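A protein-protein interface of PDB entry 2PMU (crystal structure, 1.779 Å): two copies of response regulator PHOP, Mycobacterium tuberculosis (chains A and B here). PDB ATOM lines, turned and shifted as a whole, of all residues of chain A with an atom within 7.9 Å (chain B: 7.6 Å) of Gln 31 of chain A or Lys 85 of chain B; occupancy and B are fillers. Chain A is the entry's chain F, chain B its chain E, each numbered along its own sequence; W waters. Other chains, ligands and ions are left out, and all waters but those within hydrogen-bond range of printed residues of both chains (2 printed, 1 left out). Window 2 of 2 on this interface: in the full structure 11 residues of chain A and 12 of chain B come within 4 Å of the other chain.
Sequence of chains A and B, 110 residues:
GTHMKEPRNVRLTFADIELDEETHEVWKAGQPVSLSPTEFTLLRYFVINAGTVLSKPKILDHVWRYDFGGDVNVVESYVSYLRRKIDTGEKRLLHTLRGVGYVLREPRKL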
ATOM      1  N   ASP A  16      23.626  23.846  23.289  1.00  0.00           N
ATOM      2  CA  ASP A  16      23.548  22.851  22.218  1.00  0.00           C
ATOM      3  C   ASP A  16      24.612  23.062  21.143  1.00  0.00           C
ATOM      4  O   ASP A  16      24.430  22.671  19.982  1.00  0.00           O
ATOM      5  CB  ASP A  16      22.137  22.758  21.631  1.00  0.00           C
ATOM      6  CG  ASP A  16      21.735  24.004  20.862  1.00  0.00           C
ATOM      7  OD1 ASP A  16      22.396  25.060  21.045  1.00  0.00           O
ATOM      8  OD2 ASP A  16      20.696  23.918  20.155  1.00  0.00           O
ATOM      9  N   GLU A  18      28.506  21.982  20.121  1.00  0.00           N
ATOM     10  CA  GLU A  18      29.473  20.905  20.411  1.00  0.00           C
ATOM     11  C   GLU A  18      30.681  21.046  19.520  1.00  0.00           C
ATOM     12  O   GLU A  18      30.543  21.250  18.324  1.00  0.00           O
ATOM     13  CB  GLU A  18      28.849  19.545  20.116  1.00  0.00           C
ATOM     14  CG  GLU A  18      27.608  19.225  20.897  1.00  0.00           C
ATOM     15  CD  GLU A  18      27.009  17.912  20.493  1.00  0.00           C
ATOM     16  OE1 GLU A  18      27.684  16.882  20.690  1.00  0.00           O
ATOM     17  OE2 GLU A  18      25.829  17.915  20.097  1.00  0.00           O
ATOM     18  N   VAL A  26      32.284  20.301  14.534  1.00  0.00           N
ATOM     19  CA  VAL A  26      31.344  21.151  15.284  1.00  0.00           C
ATOM     20  C   VAL A  26      29.906  20.761  14.961  1.00  0.00           C
ATOM     21  O   VAL A  26      29.599  20.390  13.801  1.00  0.00           O
ATOM     22  CB  VAL A  26      31.551  22.629  14.885  1.00  0.00           C
ATOM     23  CG1 VAL A  26      30.621  23.566  15.683  1.00  0.00           C
ATOM     24  CG2 VAL A  26      33.042  23.010  15.028  1.00  0.00           C
ATOM     25  N   TRP A  27      29.030  20.842  15.973  1.00  0.00           N
ATOM     26  CA  TRP A  27      27.580  20.622  15.782  1.00  0.00           C
ATOM     27  C   TRP A  27      26.785  21.725  16.503  1.00  0.00           C
ATOM     28  O   TRP A  27      27.201  22.201  17.521  1.00  0.00           O
ATOM     29  CB  TRP A  27      27.151  19.264  16.315  1.00  0.00           C
ATOM     30  CG  TRP A  27      27.734  18.076  15.629  1.00  0.00           C
ATOM     31  CD1 TRP A  27      27.114  17.270  14.690  1.00  0.00           C
ATOM     32  CD2 TRP A  27      29.012  17.484  15.874  1.00  0.00           C
ATOM     33  NE1 TRP A  27      27.946  16.237  14.330  1.00  0.00           N
ATOM     34  CE2 TRP A  27      29.118  16.348  15.035  1.00  0.00           C
ATOM     35  CE3 TRP A  27      30.061  17.776  16.745  1.00  0.00           C
ATOM     36  CZ2 TRP A  27      30.238  15.528  15.026  1.00  0.00           C
ATOM     37  CZ3 TRP A  27      31.191  16.970  16.720  1.00  0.00           C
ATOM     38  CH2 TRP A  27      31.272  15.861  15.863  1.00  0.00           C
ATOM     39  N   LYS A  28      25.635  22.082  15.967  1.00  0.00           N
ATOM     40  CA  LYS A  28      24.728  23.024  16.620  1.00  0.00           C
ATOM     41  C   LYS A  28      23.376  22.353  16.512  1.00  0.00           C
ATOM     42  O   LYS A  28      22.933  21.988  15.415  1.00  0.00           O
ATOM     43  CB  LYS A  28      24.770  24.382  15.861  1.00  0.00           C
ATOM     44  CG  LYS A  28      23.588  25.330  16.137  1.00  0.00           C
ATOM     45  CD  LYS A  28      23.567  25.787  17.642  1.00  0.00           C
ATOM     46  CE  LYS A  28      22.344  26.665  17.893  1.00  0.00           C
ATOM     47  NZ  LYS A  28      22.315  27.220  19.304  1.00  0.00           N
ATOM     48  N   ALA A  29      22.746  22.149  17.665  1.00  0.00           N
ATOM     49  CA  ALA A  29      21.453  21.517  17.748  1.00  0.00           C
ATOM     50  C   ALA A  29      21.532  20.134  17.084  1.00  0.00           C
ATOM     51  O   ALA A  29      20.598  19.705  16.423  1.00  0.00           O
ATOM     52  CB  ALA A  29      20.369  22.413  17.065  1.00  0.00           C
ATOM     53  N   GLY A  30      22.679  19.464  17.249  1.00  0.00           N
ATOM     54  CA  GLY A  30      22.828  18.089  16.751  1.00  0.00           C
ATOM     55  C   GLY A  30      23.213  17.990  15.276  1.00  0.00           C
ATOM     56  O   GLY A  30      23.434  16.875  14.779  1.00  0.00           O
ATOM     57  N   GLN A  31      23.283  19.130  14.582  1.00  0.00           N
ATOM     58  CA  GLN A  31      23.579  19.135  13.127  1.00  0.00           C
ATOM     59  C   GLN A  31      25.003  19.582  12.864  1.00  0.00           C
ATOM     60  O   GLN A  31      25.462  20.544  13.493  1.00  0.00           O
ATOM     61  CB  GLN A  31      22.616  20.051  12.393  1.00  0.00           C
ATOM     62  CG  GLN A  31      21.159  19.773  12.728  1.00  0.00           C
ATOM     63  CD  GLN A  31      20.654  18.497  12.095  1.00  0.00           C
ATOM     64  OE1 GLN A  31      21.427  17.703  11.527  1.00  0.00           O
ATOM     65  NE2 GLN A  31      19.349  18.293  12.162  1.00  0.00           N
ATOM     66  N   PRO A  32      25.703  18.907  11.918  1.00  0.00           N
ATOM     67  CA  PRO A  32      27.060  19.288  11.661  1.00  0.00           C
ATOM     68  C   PRO A  32      27.190  20.682  11.027  1.00  0.00           C
ATOM     69  O   PRO A  32      26.331  21.114  10.254  1.00  0.00           O
ATOM     70  CB  PRO A  32      27.537  18.240  10.659  1.00  0.00           C
ATOM     71  CG  PRO A  32      26.325  17.660  10.072  1.00  0.00           C
ATOM     72  CD  PRO A  32      25.305  17.706  11.145  1.00  0.00           C
ATOM     73  N   VAL A  33      28.284  21.335  11.364  1.00  0.00           N
ATOM     74  CA  VAL A  33      28.590  22.704  10.929  1.00  0.00           C
ATOM     75  C   VAL A  33      30.047  22.676  10.503  1.00  0.00           C
ATOM     76  O   VAL A  33      30.893  22.157  11.249  1.00  0.00           O
ATOM     77  CB  VAL A  33      28.448  23.702  12.111  1.00  0.00           C
ATOM     78  CG1 VAL A  33      28.918  25.118  11.694  1.00  0.00           C
ATOM     79  CG2 VAL A  33      27.004  23.817  12.571  1.00  0.00           C
ATOM     80  N   SER A  34      30.333  23.219   9.316  1.00  0.00           N
ATOM     81  CA  SER A  34      31.700  23.275   8.799  1.00  0.00           C
ATOM     82  C   SER A  34      32.239  24.652   9.077  1.00  0.00           C
ATOM     83  O   SER A  34      31.652  25.645   8.646  1.00  0.00           O
ATOM     84  CB  SER A  34      31.737  22.995   7.292  1.00  0.00           C
ATOM     85  OG  SER A  34      31.285  21.679   7.022  1.00  0.00           O
ATOM     86  N   LYS A  85      26.752  30.771  10.691  1.00  0.00           N
ATOM     87  CA  LYS A  85      26.833  29.327  10.646  1.00  0.00           C
ATOM     88  C   LYS A  85      26.259  28.629  11.855  1.00  0.00           C
ATOM     89  O   LYS A  85      25.759  27.498  11.730  1.00  0.00           O
ATOM     90  CB  LYS A  85      28.271  28.928  10.483  1.00  0.00           C
ATOM     91  CG  LYS A  85      28.688  29.022   9.014  1.00  0.00           C
ATOM     92  CD  LYS A  85      29.940  28.306   8.830  1.00  0.00           C
ATOM     93  CE  LYS A  85      30.563  28.604   7.509  1.00  0.00           C
ATOM     94  NZ  LYS A  85      31.998  28.232   7.586  1.00  0.00           N
ATOM     95  N   ILE A  86      26.349  29.278  13.017  1.00  0.00           N
ATOM     96  CA  ILE A  86      26.011  28.596  14.274  1.00  0.00           C
ATOM     97  C   ILE A  86      24.902  29.258  15.106  1.00  0.00           C
ATOM     98  O   ILE A  86      24.441  28.641  16.080  1.00  0.00           O
ATOM     99  CB  ILE A  86      27.283  28.421  15.136  1.00  0.00           C
ATOM    100  CG1 ILE A  86      27.187  27.117  15.924  1.00  0.00           C
ATOM    101  CG2 ILE A  86      27.566  29.625  16.013  1.00  0.00           C
ATOM    102  CD1 ILE A  86      28.500  26.570  16.391  1.00  0.00           C
ATOM    103  N   VAL B  26      25.258   5.033  13.334  1.00  0.00           N
ATOM    104  CA  VAL B  26      23.995   4.495  13.851  1.00  0.00           C
ATOM    105  C   VAL B  26      23.091   4.168  12.679  1.00  0.00           C
ATOM    106  O   VAL B  26      23.141   4.847  11.637  1.00  0.00           O
ATOM    107  CB  VAL B  26      23.299   5.601  14.747  1.00  0.00           C
ATOM    108  CG1 VAL B  26      21.843   5.153  15.167  1.00  0.00           C
ATOM    109  CG2 VAL B  26      24.218   6.008  15.959  1.00  0.00           C
ATOM    110  N   LYS B  28      18.880   2.988  11.929  1.00  0.00           N
ATOM    111  CA  LYS B  28      17.539   2.706  12.431  1.00  0.00           C
ATOM    112  C   LYS B  28      16.829   2.030  11.304  1.00  0.00           C
ATOM    113  O   LYS B  28      16.796   2.575  10.180  1.00  0.00           O
ATOM    114  CB  LYS B  28      16.840   4.031  12.812  1.00  0.00           C
ATOM    115  CG  LYS B  28      15.318   3.952  12.932  1.00  0.00           C
ATOM    116  CD  LYS B  28      14.897   3.101  14.141  1.00  0.00           C
ATOM    117  CE  LYS B  28      13.364   3.103  14.258  1.00  0.00           C
ATOM    118  NZ  LYS B  28      12.838   2.168  15.299  1.00  0.00           N
ATOM    119  N   GLN B  31      18.671   1.893   8.074  1.00  0.00           N
ATOM    120  CA  GLN B  31      19.052   3.159   7.370  1.00  0.00           C
ATOM    121  C   GLN B  31      19.982   4.015   8.246  1.00  0.00           C
ATOM    122  O   GLN B  31      19.752   4.157   9.458  1.00  0.00           O
ATOM    123  CB  GLN B  31      17.800   3.929   7.063  1.00  0.00           C
ATOM    124  CG  GLN B  31      16.805   3.184   6.191  1.00  0.00           C
ATOM    125  CD  GLN B  31      17.254   3.049   4.732  1.00  0.00           C
ATOM    126  OE1 GLN B  31      18.454   3.023   4.417  1.00  0.00           O
ATOM    127  NE2 GLN B  31      16.282   2.935   3.839  1.00  0.00           N
ATOM    128  N   PRO B  32      21.016   4.618   7.634  1.00  0.00           N
ATOM    129  CA  PRO B  32      21.959   5.338   8.469  1.00  0.00           C
ATOM    130  C   PRO B  32      21.335   6.597   9.068  1.00  0.00           C
ATOM    131  O   PRO B  32      20.530   7.315   8.413  1.00  0.00           O
ATOM    132  CB  PRO B  32      23.119   5.703   7.502  1.00  0.00           C
ATOM    133  CG  PRO B  32      22.572   5.593   6.167  1.00  0.00           C
ATOM    134  CD  PRO B  32      21.407   4.627   6.211  1.00  0.00           C
ATOM    135  N   VAL B  33      21.763   6.869  10.280  1.00  0.00           N
ATOM    136  CA  VAL B  33      21.379   8.075  11.027  1.00  0.00           C
ATOM    137  C   VAL B  33      22.644   8.776  11.497  1.00  0.00           C
ATOM    138  O   VAL B  33      23.561   8.119  12.027  1.00  0.00           O
ATOM    139  CB  VAL B  33      20.544   7.656  12.279  1.00  0.00           C
ATOM    140  CG1 VAL B  33      20.230   8.877  13.157  1.00  0.00           C
ATOM    141  CG2 VAL B  33      19.271   6.925  11.856  1.00  0.00           C
ATOM    142  N   SER B  34      22.723  10.086  11.232  1.00  0.00           N
ATOM    143  CA  SER B  34      23.841  10.889  11.697  1.00  0.00           C
ATOM    144  C   SER B  34      23.509  11.568  13.020  1.00  0.00           C
ATOM    145  O   SER B  34      22.595  12.404  13.078  1.00  0.00           O
ATOM    146  CB  SER B  34      24.192  11.945  10.654  1.00  0.00           C
ATOM    147  OG  SER B  34      24.685  11.319   9.494  1.00  0.00           O
ATOM    148  N   LEU B  35      24.255  11.215  14.064  1.00  0.00           N
ATOM    149  CA  LEU B  35      24.083  11.829  15.411  1.00  0.00           C
ATOM    150  C   LEU B  35      25.289  12.629  15.787  1.00  0.00           C
ATOM    151  O   LEU B  35      26.423  12.196  15.502  1.00  0.00           O
ATOM    152  CB  LEU B  35      23.910  10.743  16.472  1.00  0.00           C
ATOM    153  CG  LEU B  35      22.657   9.864  16.336  1.00  0.00           C
ATOM    154  CD1 LEU B  35      22.484   9.032  17.593  1.00  0.00           C
ATOM    155  CD2 LEU B  35      21.375  10.654  16.092  1.00  0.00           C
ATOM    156  N   SER B  36      25.082  13.740  16.534  1.00  0.00           N
ATOM    157  CA  SER B  36      26.216  14.487  17.120  1.00  0.00           C
ATOM    158  C   SER B  36      26.709  13.640  18.319  1.00  0.00           C
ATOM    159  O   SER B  36      26.014  12.712  18.718  1.00  0.00           O
ATOM    160  CB  SER B  36      25.752  15.849  17.612  1.00  0.00           C
ATOM    161  OG  SER B  36      24.953  15.693  18.791  1.00  0.00           O
ATOM    162  N   GLU B  39      24.070  13.546  21.111  1.00  0.00           N
ATOM    163  CA  GLU B  39      22.957  12.670  20.695  1.00  0.00           C
ATOM    164  C   GLU B  39      23.376  11.217  20.778  1.00  0.00           C
ATOM    165  O   GLU B  39      22.608  10.375  21.217  1.00  0.00           O
ATOM    166  CB  GLU B  39      22.517  13.011  19.292  1.00  0.00           C
ATOM    167  CG  GLU B  39      21.861  14.379  19.189  1.00  0.00           C
ATOM    168  CD  GLU B  39      21.546  14.736  17.736  1.00  0.00           C
ATOM    169  OE1 GLU B  39      22.242  14.233  16.791  1.00  0.00           O
ATOM    170  OE2 GLU B  39      20.601  15.535  17.549  1.00  0.00           O
ATOM    171  N   TYR B  78      17.784  18.001  23.738  1.00  0.00           N
ATOM    172  CA  TYR B  78      18.507  16.937  23.074  1.00  0.00           C
ATOM    173  C   TYR B  78      17.653  15.692  22.869  1.00  0.00           C
ATOM    174  O   TYR B  78      17.806  14.989  21.899  1.00  0.00           O
ATOM    175  CB  TYR B  78      19.796  16.583  23.812  1.00  0.00           C
ATOM    176  CG  TYR B  78      20.963  17.411  23.320  1.00  0.00           C
ATOM    177  CD1 TYR B  78      21.634  17.036  22.144  1.00  0.00           C
ATOM    178  CD2 TYR B  78      21.381  18.538  23.986  1.00  0.00           C
ATOM    179  CE1 TYR B  78      22.709  17.788  21.650  1.00  0.00           C
ATOM    180  CE2 TYR B  78      22.500  19.306  23.488  1.00  0.00           C
ATOM    181  CZ  TYR B  78      23.137  18.874  22.307  1.00  0.00           C
ATOM    182  OH  TYR B  78      24.238  19.575  21.824  1.00  0.00           O
ATOM    183  N   VAL B  79      16.707  15.456  23.763  1.00  0.00           N
ATOM    184  CA  VAL B  79      15.849  14.300  23.568  1.00  0.00           C
ATOM    185  C   VAL B  79      14.977  14.564  22.328  1.00  0.00           C
ATOM    186  O   VAL B  79      14.782  13.663  21.494  1.00  0.00           O
ATOM    187  CB  VAL B  79      15.062  13.960  24.862  1.00  0.00           C
ATOM    188  CG1 VAL B  79      13.962  12.947  24.580  1.00  0.00           C
ATOM    189  CG2 VAL B  79      16.038  13.409  25.915  1.00  0.00           C
ATOM    190  N   SER B  80      14.514  15.797  22.188  1.00  0.00           N
ATOM    191  CA  SER B  80      13.805  16.254  20.977  1.00  0.00           C
ATOM    192  C   SER B  80      14.652  16.012  19.726  1.00  0.00           C
ATOM    193  O   SER B  80      14.160  15.433  18.763  1.00  0.00           O
ATOM    194  CB  SER B  80      13.453  17.729  21.084  1.00  0.00           C
ATOM    195  OG  SER B  80      12.590  17.915  22.193  1.00  0.00           O
ATOM    196  N   TYR B  81      15.920  16.461  19.739  1.00  0.00           N
ATOM    197  CA  TYR B  81      16.764  16.319  18.535  1.00  0.00           C
ATOM    198  C   TYR B  81      16.956  14.862  18.175  1.00  0.00           C
ATOM    199  O   TYR B  81      16.875  14.452  17.003  1.00  0.00           O
ATOM    200  CB  TYR B  81      18.131  16.943  18.770  1.00  0.00           C
ATOM    201  CG  TYR B  81      18.163  18.427  19.120  1.00  0.00           C
ATOM    202  CD1 TYR B  81      17.182  19.328  18.670  1.00  0.00           C
ATOM    203  CD2 TYR B  81      19.209  18.938  19.877  1.00  0.00           C
ATOM    204  CE1 TYR B  81      17.227  20.698  19.018  1.00  0.00           C
ATOM    205  CE2 TYR B  81      19.277  20.269  20.218  1.00  0.00           C
ATOM    206  CZ  TYR B  81      18.275  21.171  19.789  1.00  0.00           C
ATOM    207  OH  TYR B  81      18.321  22.517  20.072  1.00  0.00           O
ATOM    208  N   LEU B  82      17.215  14.065  19.197  1.00  0.00           N
ATOM    209  CA  LEU B  82      17.382  12.610  19.003  1.00  0.00           C
ATOM    210  C   LEU B  82      16.106  11.927  18.471  1.00  0.00           C
ATOM    211  O   LEU B  82      16.148  11.136  17.541  1.00  0.00           O
ATOM    212  CB  LEU B  82      17.837  11.983  20.332  1.00  0.00           C
ATOM    213  CG  LEU B  82      18.060  10.468  20.329  1.00  0.00           C
ATOM    214  CD1 LEU B  82      19.155  10.094  19.295  1.00  0.00           C
ATOM    215  CD2 LEU B  82      18.415  10.018  21.733  1.00  0.00           C
ATOM    216  N   ARG B  83      14.944  12.260  19.030  1.00  0.00           N
ATOM    217  CA  ARG B  83      13.719  11.624  18.585  1.00  0.00           C
ATOM    218  C   ARG B  83      13.457  11.901  17.107  1.00  0.00           C
ATOM    219  O   ARG B  83      12.939  11.054  16.379  1.00  0.00           O
ATOM    220  CB  ARG B  83      12.539  12.162  19.374  1.00  0.00           C
ATOM    221  CG  ARG B  83      12.319  11.557  20.705  1.00  0.00           C
ATOM    222  CD  ARG B  83      11.124  12.252  21.349  1.00  0.00           C
ATOM    223  NE  ARG B  83      10.475  11.383  22.316  1.00  0.00           N
ATOM    224  CZ  ARG B  83       9.831  11.802  23.391  1.00  0.00           C
ATOM    225  NH1 ARG B  83       9.722  13.095  23.661  1.00  0.00           N
ATOM    226  NH2 ARG B  83       9.288  10.913  24.201  1.00  0.00           N
ATOM    227  N   ARG B  84      13.779  13.117  16.685  1.00  0.00           N
ATOM    228  CA  ARG B  84      13.494  13.548  15.318  1.00  0.00           C
ATOM    229  C   ARG B  84      14.317  12.711  14.339  1.00  0.00           C
ATOM    230  O   ARG B  84      13.873  12.399  13.238  1.00  0.00           O
ATOM    231  CB  ARG B  84      13.761  15.056  15.147  1.00  0.00           C
ATOM    232  CG  ARG B  84      12.777  15.919  16.009  1.00  0.00           C
ATOM    233  CD  ARG B  84      12.599  17.401  15.623  1.00  0.00           C
ATOM    234  NE  ARG B  84      13.501  18.336  16.280  1.00  0.00           N
ATOM    235  CZ  ARG B  84      13.213  19.385  17.060  1.00  0.00           C
ATOM    236  NH1 ARG B  84      14.231  20.100  17.490  1.00  0.00           N
ATOM    237  NH2 ARG B  84      11.984  19.737  17.429  1.00  0.00           N
ATOM    238  N   LYS B  85      15.492  12.308  14.782  1.00  0.00           N
ATOM    239  CA  LYS B  85      16.401  11.568  13.955  1.00  0.00           C
ATOM    240  C   LYS B  85      16.242  10.063  14.019  1.00  0.00           C
ATOM    241  O   LYS B  85      16.442   9.404  13.019  1.00  0.00           O
ATOM    242  CB  LYS B  85      17.804  11.933  14.321  1.00  0.00           C
ATOM    243  CG  LYS B  85      18.204  13.322  13.857  1.00  0.00           C
ATOM    244  CD  LYS B  85      19.680  13.405  14.128  1.00  0.00           C
ATOM    245  CE  LYS B  85      20.327  14.630  13.489  1.00  0.00           C
ATOM    246  NZ  LYS B  85      21.646  14.742  14.244  1.00  0.00           N
ATOM    247  N   ILE B  86      15.883   9.522  15.185  1.00  0.00           N
ATOM    248  CA  ILE B  86      15.915   8.081  15.371  1.00  0.00           C
ATOM    249  C   ILE B  86      14.512   7.463  15.536  1.00  0.00           C
ATOM    250  O   ILE B  86      14.373   6.246  15.462  1.00  0.00           O
ATOM    251  CB  ILE B  86      16.775   7.688  16.604  1.00  0.00           C
ATOM    252  CG1 ILE B  86      17.251   6.216  16.512  1.00  0.00           C
ATOM    253  CG2 ILE B  86      15.993   7.896  17.941  1.00  0.00           C
ATOM    254  CD1 ILE B  86      18.661   6.055  16.065  1.00  0.00           C
ATOM    255  N   ASP B  87      13.503   8.277  15.805  1.00  0.00           N
ATOM    256  CA  ASP B  87      12.199   7.738  16.272  1.00  0.00           C
ATOM    257  C   ASP B  87      11.016   8.347  15.548  1.00  0.00           C
ATOM    258  O   ASP B  87      10.073   8.842  16.180  1.00  0.00           O
ATOM    259  CB  ASP B  87      12.055   7.940  17.803  1.00  0.00           C
ATOM    260  CG  ASP B  87      11.173   6.897  18.447  1.00  0.00           C
ATOM    261  OD1 ASP B  87      11.212   5.718  18.004  1.00  0.00           O
ATOM    262  OD2 ASP B  87      10.418   7.256  19.390  1.00  0.00           O
ATOM    263  N   THR B  88      11.066   8.301  14.221  1.00  0.00           N
ATOM    264  CA  THR B  88      10.053   8.942  13.389  1.00  0.00           C
ATOM    265  C   THR B  88       9.066   7.936  12.819  1.00  0.00           C
ATOM    266  O   THR B  88       7.981   8.322  12.355  1.00  0.00           O
ATOM    267  CB  THR B  88      10.678   9.779  12.245  1.00  0.00           C
ATOM    268  OG1 THR B  88      11.759   9.054  11.644  1.00  0.00           O
ATOM    269  CG2 THR B  88      11.210  11.104  12.787  1.00  0.00           C
ATOM    270  N   GLY B  89       9.449   6.659  12.847  1.00  0.00           N
ATOM    271  CA  GLY B  89       8.540   5.541  12.507  1.00  0.00           C
ATOM    272  C   GLY B  89       7.175   5.528  13.206  1.00  0.00           C
ATOM    273  O   GLY B  89       6.901   6.339  14.099  1.00  0.00           O
HETATM  274  O   HOH W   1      24.557  15.020  12.822  1.00  0.00           O
HETATM  275  O   HOH W   2      19.746  17.173  15.467  1.00  0.00           O
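OG of Ser 36 of chain B lies within hydrogen-bond range of OE2 of Glu 18 of chain A, at 2.7 Å. The side-chain hydroxyl of Tyr 78 of chain B is in hydrogen-bond range of the side-chain carboxylate of Glu 18 of chain A (2.9 Å). The side-chain carboxylate of Asp 16 of chain A sits at hydrogen-bond distance from the side-chain hydroxyl of Tyr 81 of chain B, at 2.8 Å. The side-chain amino group (NZ) of Lys 85 of chain B lies within hydrogen-bond range of the backbone carbonyl oxygen (O) of Gly 30 of chain A, 2.8 Å away.
Among the printed residues, merely in contact across the chains: Asp 16 of chain A with Tyr 78 of chain B, Gly 30 of chain A with Glu 39 of chain B, Ala 29 of chain A with Tyr 81 of chain B, Trp 27 of chain A with Ser 36 of chain B, Gly 30 of chain A with Ser 36 of chain B and Gln 31 of chain A with Lys 85 of chain B.
Of chain B, only Lys 85 comes within 4 Å of Gln 31 of chain A. Of chain A, only Gly 30 and Gln 31 come within 4 Å of Lys 85 of chain B. Gly 30 of chain A touches just these residues of chain B: Ser 36 (3.8 Å), Glu 39 (3.5 Å) and Lys 85 (2.8 Å). Printed residues of chain B within 4 Å of Trp 27 of chain A: Ser 36. Of the printed residues of chain A, Tyr 78 of chain B touches Asp 16 and Glu 18. Of the printed residues of chain A, Glu 39 of chain B touches Gly 30. Of the printed residues of chain A, Ser 36 of chain B touches Glu 18, Trp 27 and Gly 30. Gly 89 of chain B touches none of the printed residues of chain A. Asp 87 of chain B touches none of the printed residues of chain A. The nearest residue of chain B that does not touch Gln 31 of chain A is Ser 36 of chain B (5.1 Å). The nearest residue of chain A that does not touch Lys 85 of chain B is Ala 29 of chain A (5.5 Å). The nearest printed residue of chain A that does not touch Ser 36 of chain B is Gln 31 of chain A (5.1 Å).
The backbone carbonyl oxygen of Ser 34 of chain B lies within hydrogen-bond range of the side-chain amino group of Lys 85 of chain B, 2.8 Å away. OE1 of Glu 39 of chain B lies within hydrogen-bond range of N of Ser 36 of chain B (2.9 Å). The side-chain amino group of Lys 85 of chain B is in salt-bridge range of the side-chain carboxylate of Glu 39 of chain B, at 2.7 Å. The side-chain carboxylate (OD1) of Asp 16 of chain A lies within salt-bridge range of the side-chain amino group (NZ) of Lys 28 of chain A. The backbone carbonyl oxygen (O) of Asp 16 of chain A lies within hydrogen-bond range of the backbone NH (N) of Ala 29 of chain A (2.9 Å). The backbone carbonyl oxygen of Glu 18 of chain A is in hydrogen-bond range of the backbone NH of Trp 27 of chain A, 2.8 Å away.
Gln 31 of chain A touches Lys 85 of chain B, but with the chains exchanged Lys 85 of chain A does not touch Gln 31 of chain B (24.2 Å). Positions printed for both chains: 26, 28, 31, 32, 33, 34, 85 and 86.
Water W2 lies within hydrogen-bond range of the side-chain carboxylate (OE2) of Glu 39 of chain B, the backbone carbonyl oxygen (O) of Ala 29 of chain A and the side-chain amino group (NZ) of Lys 85 of chain B. Water W1 lies within hydrogen-bond range of O of Gly 30 of chain A, NZ of Lys 85 of chain B and O of Ser 34 of chain B.
Of the 21 printed residues of chain B, 5 touch a printed residue of chain A. Hydrophobic or aromatic side chains of chain B within 4 Å of the printed part of chain A: Tyr 78 and Tyr 81. Printed residues of chain A that touch a printed residue of chain B: Asp 16, Glu 18, Trp 27, Ala 29, Gly 30 and Gln 31. Hydrophobic or aromatic side chains of chain A that line the printed part of chain B: Trp 27 and Ala 29. Among the printed residues, no Asp or Glu carboxylate lies within 4 Å of a Lys or Arg side-chain nitrogen of the other chain.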
